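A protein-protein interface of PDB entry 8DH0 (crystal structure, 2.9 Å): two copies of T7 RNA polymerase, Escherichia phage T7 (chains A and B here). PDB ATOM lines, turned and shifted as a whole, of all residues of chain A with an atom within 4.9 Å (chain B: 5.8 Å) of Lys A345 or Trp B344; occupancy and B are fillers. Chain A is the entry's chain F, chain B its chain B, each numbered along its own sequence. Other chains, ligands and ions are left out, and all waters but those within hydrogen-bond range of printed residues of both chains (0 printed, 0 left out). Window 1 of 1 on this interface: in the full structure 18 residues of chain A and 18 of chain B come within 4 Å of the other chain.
The backbone carbonyl oxygen (O) of Trp B344 is in hydrogen-bond range of the side-chain amino group (NZ) of Lys A345 (3.5 Å).
The indole nitrogen of Trp B344 is in hydrogen-bond range of the backbone carbonyl oxygen of Leu A497 (3.1 Å).
The side-chain amino group of Lys B345 lies within hydrogen-bond range of the backbone carbonyl oxygen of Trp A344 (3.2 Å).
O of Trp A344 lies close to O of Asp B351, at 3.1 Å.
O of Trp B344 sits close to O of Asp A351 (3.0 Å).
NZ of Lys B345 sits at hydrogen-bond distance from O of Asp B351 (2.8 Å).
The side-chain amino group (NZ) of Lys A345 lies within hydrogen-bond range of the backbone carbonyl oxygen (O) of Pro A348 (3.3 Å).
The side-chain amino group (NZ) of Lys A345 lies within hydrogen-bond range of the backbone carbonyl oxygen (O) of Asp A351, 2.5 Å away.
O of Lys A345 lies within hydrogen-bond range of NH1 of Arg A395, at 2.7 Å.
O of Pro A496 is in hydrogen-bond range of NE1 of Trp A502 (3.0 Å).
O of Asn A499 sits close to NE1 of Trp A502 (3.4 Å).
Lys A343 touches Ile B352 (O to CG2, 3.7 Å).
CE3 of Trp A344 touches CD1 of Ile B352, at 3.5 Å.
Pro B353 touches Trp A344.
Pro B353 touches Lys A345.
CG of Pro B353 touches N of His A346, 3.5 Å away.
O of Lys B343 touches CD of Pro A353, at 3.4 Å.
Lys B345 touches Pro A353.
Arg A395 touches Pro B353.
CZ2 of Trp A502 touches CH2 of Trp B344, 3.6 Å away.
Trp B344 touches Ala A503.
Ile A341 touches none of the printed residues of chain B.
Of the printed residues of chain B, Lys A345 touches Trp B344 and Pro B353.
Glu A350 touches none of the printed residues of chain B.
Of the printed residues of chain B, Asp A351 touches Trp B344.
Of the printed residues of chain A, Thr B342 touches Pro A353 (3.7 Å).
Printed residues of chain A within 4 Å of Trp B344: Lys A345, Asp A351, Ile A352, Pro A353, Pro A496, Leu A497, Thr A500, Trp A502 and Ala A503.
Printed residues of chain A within 4 Å of His B346: Pro A353 (3.5 Å).
Of the printed residues of chain A, Pro B353 touches Thr A342, Lys A343, Trp A344, Lys A345, His A346 and Arg A395.
The nearest residue of chain B that does not touch Lys A345 is Lys B345 (4.3 Å).
The nearest printed residue of chain A that does not touch Lys B343 is Asn A499 (5.2 Å).
Of the 10 printed residues of chain B, 9 touch a printed residue of chain A.
Printed residues of chain B that touch a printed residue of chain A: Val B340, Thr B342, Lys B343, Trp B344, Lys B345, His B346, Asp B351, Ile B352 and Pro B353.
Hydrophobic or aromatic side chains of chain B within 4 Å of the printed part of chain A: Val B340, Trp B344, His B346, Ile B352 and Pro B353.
Of the 20 printed residues of chain A, 14 touch a printed residue of chain B.
Hydrophobic or aromatic side chains of chain A that line the printed part of chain B: Trp A344, His A346, Ile A352, Pro A353, Trp A502 and Ala A503.
Thr A342 touches Pro B353, and with the chains exchanged Pro A353 touches Thr B342.
Lys A343 touches Pro B353, and with the chains exchanged Pro A353 touches Lys B343.
Trp A344 touches Ile B352, and with the chains exchanged Ile A352 touches Trp B344.
Trp A344 touches Pro B353, and with the chains exchanged Pro A353 touches Trp B344.
Of the 26 pairs that touch across the chains among the printed residues, 18 have their exchanged pair printed and touching as well.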
ATOM      1  N   ILE A 341      17.574 -11.925 -23.846  1.00  0.00           N
ATOM      2  CA  ILE A 341      16.586 -12.049 -22.777  1.00  0.00           C
ATOM      3  C   ILE A 341      15.210 -12.408 -23.320  1.00  0.00           C
ATOM      4  O   ILE A 341      14.377 -12.950 -22.585  1.00  0.00           O
ATOM      5  CB  ILE A 341      16.520 -10.749 -21.945  1.00  0.00           C
ATOM      6  CG1 ILE A 341      16.747  -9.538 -22.844  1.00  0.00           C
ATOM      7  CG2 ILE A 341      17.546 -10.771 -20.825  1.00  0.00           C
ATOM      8  CD1 ILE A 341      16.448  -8.214 -22.190  1.00  0.00           C
ATOM      9  N   THR A 342      14.953 -12.121 -24.597  1.00  0.00           N
ATOM     10  CA  THR A 342      13.663 -12.453 -25.193  1.00  0.00           C
ATOM     11  C   THR A 342      13.499 -13.960 -25.367  1.00  0.00           C
ATOM     12  O   THR A 342      12.415 -14.502 -25.121  1.00  0.00           O
ATOM     13  CB  THR A 342      13.508 -11.721 -26.528  1.00  0.00           C
ATOM     14  OG1 THR A 342      13.022 -10.394 -26.287  1.00  0.00           O
ATOM     15  CG2 THR A 342      12.557 -12.448 -27.464  1.00  0.00           C
ATOM     16  N   LYS A 343      14.565 -14.660 -25.770  1.00  0.00           N
ATOM     17  CA  LYS A 343      14.483 -16.111 -25.911  1.00  0.00           C
ATOM     18  C   LYS A 343      14.201 -16.801 -24.586  1.00  0.00           C
ATOM     19  O   LYS A 343      13.673 -17.919 -24.579  1.00  0.00           O
ATOM     20  CB  LYS A 343      15.775 -16.684 -26.498  1.00  0.00           C
ATOM     21  CG  LYS A 343      16.213 -16.089 -27.821  1.00  0.00           C
ATOM     22  CD  LYS A 343      17.728 -16.147 -27.948  1.00  0.00           C
ATOM     23  CE  LYS A 343      18.176 -15.989 -29.391  1.00  0.00           C
ATOM     24  NZ  LYS A 343      18.395 -17.308 -30.046  1.00  0.00           N
ATOM     25  N   TRP A 344      14.538 -16.163 -23.468  1.00  0.00           N
ATOM     26  CA  TRP A 344      14.396 -16.775 -22.155  1.00  0.00           C
ATOM     27  C   TRP A 344      13.120 -16.375 -21.437  1.00  0.00           C
ATOM     28  O   TRP A 344      12.618 -17.147 -20.615  1.00  0.00           O
ATOM     29  CB  TRP A 344      15.600 -16.412 -21.281  1.00  0.00           C
ATOM     30  CG  TRP A 344      16.840 -17.124 -21.694  1.00  0.00           C
ATOM     31  CD1 TRP A 344      17.858 -16.628 -22.452  1.00  0.00           C
ATOM     32  CD2 TRP A 344      17.189 -18.475 -21.385  1.00  0.00           C
ATOM     33  NE1 TRP A 344      18.826 -17.587 -22.630  1.00  0.00           N
ATOM     34  CE2 TRP A 344      18.438 -18.731 -21.983  1.00  0.00           C
ATOM     35  CE3 TRP A 344      16.569 -19.492 -20.657  1.00  0.00           C
ATOM     36  CZ2 TRP A 344      19.076 -19.962 -21.875  1.00  0.00           C
ATOM     37  CZ3 TRP A 344      17.202 -20.711 -20.551  1.00  0.00           C
ATOM     38  CH2 TRP A 344      18.441 -20.937 -21.156  1.00  0.00           C
ATOM     39  N   LYS A 345      12.576 -15.197 -21.733  1.00  0.00           N
ATOM     40  CA  LYS A 345      11.421 -14.667 -21.026  1.00  0.00           C
ATOM     41  C   LYS A 345      10.377 -14.188 -22.022  1.00  0.00           C
ATOM     42  O   LYS A 345      10.719 -13.632 -23.068  1.00  0.00           O
ATOM     43  CB  LYS A 345      11.828 -13.515 -20.112  1.00  0.00           C
ATOM     44  CG  LYS A 345      12.844 -13.888 -19.051  1.00  0.00           C
ATOM     45  CD  LYS A 345      12.977 -12.752 -18.076  1.00  0.00           C
ATOM     46  CE  LYS A 345      11.692 -12.626 -17.296  1.00  0.00           C
ATOM     47  NZ  LYS A 345      11.713 -11.455 -16.407  1.00  0.00           N
ATOM     48  N   HIS A 346       9.100 -14.418 -21.697  1.00  0.00           N
ATOM     49  CA  HIS A 346       8.022 -13.936 -22.557  1.00  0.00           C
ATOM     50  C   HIS A 346       8.061 -12.418 -22.671  1.00  0.00           C
ATOM     51  O   HIS A 346       8.073 -11.864 -23.777  1.00  0.00           O
ATOM     52  CB  HIS A 346       6.672 -14.414 -22.024  1.00  0.00           C
ATOM     53  CG  HIS A 346       6.284 -15.776 -22.508  1.00  0.00           C
ATOM     54  ND1 HIS A 346       6.494 -16.916 -21.765  1.00  0.00           N
ATOM     55  CD2 HIS A 346       5.709 -16.180 -23.665  1.00  0.00           C
ATOM     56  CE1 HIS A 346       6.061 -17.966 -22.440  1.00  0.00           C
ATOM     57  NE2 HIS A 346       5.579 -17.547 -23.597  1.00  0.00           N
ATOM     58  N   CYS A 347       8.095 -11.728 -21.537  1.00  0.00           N
ATOM     59  CA  CYS A 347       8.469 -10.327 -21.522  1.00  0.00           C
ATOM     60  C   CYS A 347       9.783 -10.182 -20.777  1.00  0.00           C
ATOM     61  O   CYS A 347       9.903 -10.673 -19.645  1.00  0.00           O
ATOM     62  CB  CYS A 347       7.392  -9.462 -20.865  1.00  0.00           C
ATOM     63  SG  CYS A 347       7.825  -7.704 -20.756  1.00  0.00           S
ATOM     64  N   PRO A 348      10.784  -9.541 -21.383  1.00  0.00           N
ATOM     65  CA  PRO A 348      12.136  -9.548 -20.797  1.00  0.00           C
ATOM     66  C   PRO A 348      12.225  -8.942 -19.405  1.00  0.00           C
ATOM     67  O   PRO A 348      13.034  -9.407 -18.592  1.00  0.00           O
ATOM     68  CB  PRO A 348      12.951  -8.736 -21.813  1.00  0.00           C
ATOM     69  CG  PRO A 348      12.183  -8.847 -23.093  1.00  0.00           C
ATOM     70  CD  PRO A 348      10.746  -8.847 -22.679  1.00  0.00           C
ATOM     71  N   VAL A 349      11.425  -7.925 -19.104  1.00  0.00           N
ATOM     72  CA  VAL A 349      11.525  -7.199 -17.846  1.00  0.00           C
ATOM     73  C   VAL A 349      10.346  -7.488 -16.925  1.00  0.00           C
ATOM     74  O   VAL A 349      10.213  -6.845 -15.878  1.00  0.00           O
ATOM     75  CB  VAL A 349      11.664  -5.687 -18.094  1.00  0.00           C
ATOM     76  CG1 VAL A 349      12.877  -5.404 -18.965  1.00  0.00           C
ATOM     77  CG2 VAL A 349      10.402  -5.143 -18.737  1.00  0.00           C
ATOM     78  N   GLU A 350       9.487  -8.445 -17.283  1.00  0.00           N
ATOM     79  CA  GLU A 350       8.225  -8.617 -16.566  1.00  0.00           C
ATOM     80  C   GLU A 350       8.441  -9.136 -15.148  1.00  0.00           C
ATOM     81  O   GLU A 350       7.944  -8.548 -14.181  1.00  0.00           O
ATOM     82  CB  GLU A 350       7.305  -9.555 -17.346  1.00  0.00           C
ATOM     83  CG  GLU A 350       5.827  -9.343 -17.073  1.00  0.00           C
ATOM     84  CD  GLU A 350       5.042 -10.639 -17.074  1.00  0.00           C
ATOM     85  OE1 GLU A 350       4.113 -10.776 -16.249  1.00  0.00           O
ATOM     86  OE2 GLU A 350       5.354 -11.518 -17.903  1.00  0.00           O
ATOM     87  N   ASP A 351       9.187 -10.230 -15.000  1.00  0.00           N
ATOM     88  CA  ASP A 351       9.395 -10.861 -13.696  1.00  0.00           C
ATOM     89  C   ASP A 351      10.889 -11.069 -13.474  1.00  0.00           C
ATOM     90  O   ASP A 351      11.472 -12.037 -13.975  1.00  0.00           O
ATOM     91  CB  ASP A 351       8.638 -12.182 -13.592  1.00  0.00           C
ATOM     92  CG  ASP A 351       7.195 -11.995 -13.160  1.00  0.00           C
ATOM     93  OD1 ASP A 351       6.950 -11.875 -11.941  1.00  0.00           O
ATOM     94  OD2 ASP A 351       6.304 -11.981 -14.036  1.00  0.00           O
ATOM     95  N   ILE A 352      11.501 -10.162 -12.725  1.00  0.00           N
ATOM     96  CA  ILE A 352      12.900 -10.274 -12.322  1.00  0.00           C
ATOM     97  C   ILE A 352      12.920 -10.705 -10.860  1.00  0.00           C
ATOM     98  O   ILE A 352      12.277 -10.046 -10.028  1.00  0.00           O
ATOM     99  CB  ILE A 352      13.655  -8.949 -12.504  1.00  0.00           C
ATOM    100  CG1 ILE A 352      13.675  -8.508 -13.970  1.00  0.00           C
ATOM    101  CG2 ILE A 352      15.083  -9.087 -11.994  1.00  0.00           C
ATOM    102  CD1 ILE A 352      13.909  -9.622 -14.942  1.00  0.00           C
ATOM    103  N   PRO A 353      13.595 -11.798 -10.509  1.00  0.00           N
ATOM    104  CA  PRO A 353      13.757 -12.131  -9.091  1.00  0.00           C
ATOM    105  C   PRO A 353      14.465 -11.008  -8.348  1.00  0.00           C
ATOM    106  O   PRO A 353      15.399 -10.389  -8.863  1.00  0.00           O
ATOM    107  CB  PRO A 353      14.603 -13.407  -9.122  1.00  0.00           C
ATOM    108  CG  PRO A 353      14.283 -14.023 -10.434  1.00  0.00           C
ATOM    109  CD  PRO A 353      14.070 -12.880 -11.388  1.00  0.00           C
ATOM    110  N   ARG A 395       3.488 -10.388 -26.461  1.00  0.00           N
ATOM    111  CA  ARG A 395       4.593 -11.085 -27.111  1.00  0.00           C
ATOM    112  C   ARG A 395       4.537 -10.945 -28.627  1.00  0.00           C
ATOM    113  O   ARG A 395       5.571 -10.722 -29.265  1.00  0.00           O
ATOM    114  CB  ARG A 395       4.595 -12.559 -26.707  1.00  0.00           C
ATOM    115  CG  ARG A 395       5.687 -13.385 -27.373  1.00  0.00           C
ATOM    116  CD  ARG A 395       6.848 -13.642 -26.424  1.00  0.00           C
ATOM    117  NE  ARG A 395       7.995 -14.227 -27.110  1.00  0.00           N
ATOM    118  CZ  ARG A 395       9.241 -14.188 -26.659  1.00  0.00           C
ATOM    119  NH1 ARG A 395       9.549 -13.581 -25.524  1.00  0.00           N
ATOM    120  NH2 ARG A 395      10.203 -14.774 -27.364  1.00  0.00           N
ATOM    121  N   PRO A 496      25.538  -6.382 -19.535  1.00  0.00           N
ATOM    122  CA  PRO A 496      24.089  -6.180 -19.367  1.00  0.00           C
ATOM    123  C   PRO A 496      23.326  -7.434 -18.975  1.00  0.00           C
ATOM    124  O   PRO A 496      22.277  -7.329 -18.326  1.00  0.00           O
ATOM    125  CB  PRO A 496      23.649  -5.662 -20.743  1.00  0.00           C
ATOM    126  CG  PRO A 496      24.916  -5.213 -21.425  1.00  0.00           C
ATOM    127  CD  PRO A 496      25.971  -6.137 -20.919  1.00  0.00           C
ATOM    128  N   LEU A 497      23.804  -8.617 -19.357  1.00  0.00           N
ATOM    129  CA  LEU A 497      23.154  -9.849 -18.935  1.00  0.00           C
ATOM    130  C   LEU A 497      23.596 -10.306 -17.552  1.00  0.00           C
ATOM    131  O   LEU A 497      23.023 -11.263 -17.022  1.00  0.00           O
ATOM    132  CB  LEU A 497      23.421 -10.964 -19.947  1.00  0.00           C
ATOM    133  CG  LEU A 497      23.153 -10.648 -21.418  1.00  0.00           C
ATOM    134  CD1 LEU A 497      23.420 -11.873 -22.270  1.00  0.00           C
ATOM    135  CD2 LEU A 497      21.727 -10.161 -21.607  1.00  0.00           C
ATOM    136  N   ASN A 499      24.124  -7.931 -14.828  1.00  0.00           N
ATOM    137  CA  ASN A 499      23.538  -7.045 -13.829  1.00  0.00           C
ATOM    138  C   ASN A 499      22.156  -6.629 -14.309  1.00  0.00           C
ATOM    139  O   ASN A 499      22.027  -6.001 -15.365  1.00  0.00           O
ATOM    140  CB  ASN A 499      24.422  -5.820 -13.579  1.00  0.00           C
ATOM    141  CG  ASN A 499      25.903  -6.145 -13.648  1.00  0.00           C
ATOM    142  OD1 ASN A 499      26.480  -6.242 -14.730  1.00  0.00           O
ATOM    143  ND2 ASN A 499      26.524  -6.325 -12.487  1.00  0.00           N
ATOM    144  N   THR A 500      21.134  -6.973 -13.533  1.00  0.00           N
ATOM    145  CA  THR A 500      19.746  -6.763 -13.922  1.00  0.00           C
ATOM    146  C   THR A 500      19.189  -5.424 -13.458  1.00  0.00           C
ATOM    147  O   THR A 500      17.987  -5.188 -13.617  1.00  0.00           O
ATOM    148  CB  THR A 500      18.867  -7.894 -13.375  1.00  0.00           C
ATOM    149  OG1 THR A 500      18.748  -7.768 -11.952  1.00  0.00           O
ATOM    150  CG2 THR A 500      19.475  -9.250 -13.710  1.00  0.00           C
ATOM    151  N   TRP A 502      19.294  -2.434 -14.575  1.00  0.00           N
ATOM    152  CA  TRP A 502      18.633  -1.635 -15.602  1.00  0.00           C
ATOM    153  C   TRP A 502      17.226  -2.148 -15.886  1.00  0.00           C
ATOM    154  O   TRP A 502      16.304  -1.355 -16.110  1.00  0.00           O
ATOM    155  CB  TRP A 502      19.474  -1.610 -16.879  1.00  0.00           C
ATOM    156  CG  TRP A 502      19.643  -2.944 -17.542  1.00  0.00           C
ATOM    157  CD1 TRP A 502      20.667  -3.825 -17.358  1.00  0.00           C
ATOM    158  CD2 TRP A 502      18.768  -3.542 -18.507  1.00  0.00           C
ATOM    159  NE1 TRP A 502      20.484  -4.937 -18.144  1.00  0.00           N
ATOM    160  CE2 TRP A 502      19.324  -4.787 -18.858  1.00  0.00           C
ATOM    161  CE3 TRP A 502      17.567  -3.147 -19.105  1.00  0.00           C
ATOM    162  CZ2 TRP A 502      18.720  -5.640 -19.779  1.00  0.00           C
ATOM    163  CZ3 TRP A 502      16.969  -3.996 -20.018  1.00  0.00           C
ATOM    164  CH2 TRP A 502      17.547  -5.227 -20.347  1.00  0.00           C
ATOM    165  N   ALA A 503      17.039  -3.471 -15.876  1.00  0.00           N
ATOM    166  CA  ALA A 503      15.725  -4.046 -16.145  1.00  0.00           C
ATOM    167  C   ALA A 503      14.701  -3.675 -15.081  1.00  0.00           C
ATOM    168  O   ALA A 503      13.496  -3.733 -15.348  1.00  0.00           O
ATOM    169  CB  ALA A 503      15.828  -5.567 -16.257  1.00  0.00           C
ATOM    170  N   VAL B 340      23.782 -16.742 -14.274  1.00  0.00           N
ATOM    171  CA  VAL B 340      23.193 -15.687 -15.092  1.00  0.00           C
ATOM    172  C   VAL B 340      21.676 -15.811 -15.131  1.00  0.00           C
ATOM    173  O   VAL B 340      20.951 -14.903 -14.706  1.00  0.00           O
ATOM    174  CB  VAL B 340      23.790 -15.713 -16.508  1.00  0.00           C
ATOM    175  CG1 VAL B 340      23.152 -14.631 -17.358  1.00  0.00           C
ATOM    176  CG2 VAL B 340      25.298 -15.540 -16.450  1.00  0.00           C
ATOM    177  N   ILE B 341      21.181 -16.942 -15.637  1.00  0.00           N
ATOM    178  CA  ILE B 341      19.752 -17.130 -15.879  1.00  0.00           C
ATOM    179  C   ILE B 341      18.946 -17.066 -14.590  1.00  0.00           C
ATOM    180  O   ILE B 341      17.783 -16.639 -14.597  1.00  0.00           O
ATOM    181  CB  ILE B 341      19.552 -18.454 -16.643  1.00  0.00           C
ATOM    182  CG1 ILE B 341      20.269 -19.611 -15.951  1.00  0.00           C
ATOM    183  CG2 ILE B 341      20.048 -18.340 -18.056  1.00  0.00           C
ATOM    184  CD1 ILE B 341      19.949 -20.962 -16.558  1.00  0.00           C
ATOM    185  N   THR B 342      19.546 -17.465 -13.468  1.00  0.00           N
ATOM    186  CA  THR B 342      18.844 -17.421 -12.188  1.00  0.00           C
ATOM    187  C   THR B 342      18.475 -15.992 -11.807  1.00  0.00           C
ATOM    188  O   THR B 342      17.401 -15.746 -11.246  1.00  0.00           O
ATOM    189  CB  THR B 342      19.712 -18.076 -11.111  1.00  0.00           C
ATOM    190  OG1 THR B 342      19.558 -19.500 -11.180  1.00  0.00           O
ATOM    191  CG2 THR B 342      19.369 -17.578  -9.714  1.00  0.00           C
ATOM    192  N   LYS B 343      19.342 -15.032 -12.131  1.00  0.00           N
ATOM    193  CA  LYS B 343      19.044 -13.635 -11.846  1.00  0.00           C
ATOM    194  C   LYS B 343      17.869 -13.109 -12.662  1.00  0.00           C
ATOM    195  O   LYS B 343      17.256 -12.113 -12.264  1.00  0.00           O
ATOM    196  CB  LYS B 343      20.282 -12.778 -12.103  1.00  0.00           C
ATOM    197  CG  LYS B 343      21.437 -13.084 -11.167  1.00  0.00           C
ATOM    198  CD  LYS B 343      22.385 -11.904 -11.060  1.00  0.00           C
ATOM    199  CE  LYS B 343      23.631 -12.141 -11.889  1.00  0.00           C
ATOM    200  NZ  LYS B 343      24.557 -13.112 -11.249  1.00  0.00           N
ATOM    201  N   TRP B 344      17.537 -13.755 -13.779  1.00  0.00           N
ATOM    202  CA  TRP B 344      16.492 -13.269 -14.671  1.00  0.00           C
ATOM    203  C   TRP B 344      15.154 -13.972 -14.488  1.00  0.00           C
ATOM    204  O   TRP B 344      14.109 -13.353 -14.719  1.00  0.00           O
ATOM    205  CB  TRP B 344      16.944 -13.407 -16.130  1.00  0.00           C
ATOM    206  CG  TRP B 344      17.994 -12.407 -16.513  1.00  0.00           C
ATOM    207  CD1 TRP B 344      19.337 -12.624 -16.613  1.00  0.00           C
ATOM    208  CD2 TRP B 344      17.785 -11.028 -16.837  1.00  0.00           C
ATOM    209  NE1 TRP B 344      19.977 -11.464 -16.981  1.00  0.00           N
ATOM    210  CE2 TRP B 344      19.046 -10.470 -17.125  1.00  0.00           C
ATOM    211  CE3 TRP B 344      16.656 -10.212 -16.915  1.00  0.00           C
ATOM    212  CZ2 TRP B 344      19.206  -9.133 -17.484  1.00  0.00           C
ATOM    213  CZ3 TRP B 344      16.815  -8.886 -17.267  1.00  0.00           C
ATOM    214  CH2 TRP B 344      18.080  -8.359 -17.549  1.00  0.00           C
ATOM    215  N   LYS B 345      15.152 -15.240 -14.083  1.00  0.00           N
ATOM    216  CA  LYS B 345      13.929 -16.010 -13.905  1.00  0.00           C
ATOM    217  C   LYS B 345      13.920 -16.662 -12.529  1.00  0.00           C
ATOM    218  O   LYS B 345      14.969 -17.043 -12.004  1.00  0.00           O
ATOM    219  CB  LYS B 345      13.782 -17.090 -14.985  1.00  0.00           C
ATOM    220  CG  LYS B 345      14.463 -16.754 -16.301  1.00  0.00           C
ATOM    221  CD  LYS B 345      14.114 -17.762 -17.376  1.00  0.00           C
ATOM    222  CE  LYS B 345      12.613 -17.927 -17.499  1.00  0.00           C
ATOM    223  NZ  LYS B 345      12.268 -19.186 -18.200  1.00  0.00           N
ATOM    224  N   HIS B 346      12.725 -16.771 -11.940  1.00  0.00           N
ATOM    225  CA  HIS B 346      12.599 -17.434 -10.644  1.00  0.00           C
ATOM    226  C   HIS B 346      13.003 -18.898 -10.740  1.00  0.00           C
ATOM    227  O   HIS B 346      13.862 -19.371  -9.988  1.00  0.00           O
ATOM    228  CB  HIS B 346      11.169 -17.302 -10.119  1.00  0.00           C
ATOM    229  CG  HIS B 346      10.890 -15.995  -9.451  1.00  0.00           C
ATOM    230  ND1 HIS B 346       9.944 -15.106  -9.916  1.00  0.00           N
ATOM    231  CD2 HIS B 346      11.435 -15.422  -8.351  1.00  0.00           C
ATOM    232  CE1 HIS B 346       9.918 -14.043  -9.131  1.00  0.00           C
ATOM    233  NE2 HIS B 346      10.813 -14.210  -8.174  1.00  0.00           N
ATOM    234  N   ASP B 351       9.685 -21.165 -17.716  1.00  0.00           N
ATOM    235  CA  ASP B 351       8.869 -20.599 -18.789  1.00  0.00           C
ATOM    236  C   ASP B 351       9.783 -20.093 -19.897  1.00  0.00           C
ATOM    237  O   ASP B 351      10.085 -18.901 -19.985  1.00  0.00           O
ATOM    238  CB  ASP B 351       7.972 -19.488 -18.249  1.00  0.00           C
ATOM    239  CG  ASP B 351       6.698 -20.023 -17.633  1.00  0.00           C
ATOM    240  OD1 ASP B 351       6.049 -20.883 -18.265  1.00  0.00           O
ATOM    241  OD2 ASP B 351       6.349 -19.589 -16.514  1.00  0.00           O
ATOM    242  N   ILE B 352      10.199 -21.007 -20.762  1.00  0.00           N
ATOM    243  CA  ILE B 352      10.892 -20.625 -21.992  1.00  0.00           C
ATOM    244  C   ILE B 352       9.841 -20.291 -23.047  1.00  0.00           C
ATOM    245  O   ILE B 352       8.927 -21.099 -23.272  1.00  0.00           O
ATOM    246  CB  ILE B 352      11.805 -21.751 -22.474  1.00  0.00           C
ATOM    247  CG1 ILE B 352      12.754 -22.225 -21.369  1.00  0.00           C
ATOM    248  CG2 ILE B 352      12.609 -21.297 -23.687  1.00  0.00           C
ATOM    249  CD1 ILE B 352      13.455 -21.116 -20.626  1.00  0.00           C
ATOM    250  N   PRO B 353       9.899 -19.117 -23.672  1.00  0.00           N
ATOM    251  CA  PRO B 353       9.056 -18.881 -24.846  1.00  0.00           C
ATOM    252  C   PRO B 353       9.336 -19.920 -25.918  1.00  0.00           C
ATOM    253  O   PRO B 353      10.489 -20.253 -26.204  1.00  0.00           O
ATOM    254  CB  PRO B 353       9.464 -17.477 -25.300  1.00  0.00           C
ATOM    255  CG  PRO B 353       9.922 -16.818 -24.060  1.00  0.00           C
ATOM    256  CD  PRO B 353      10.582 -17.889 -23.231  1.00  0.00           C
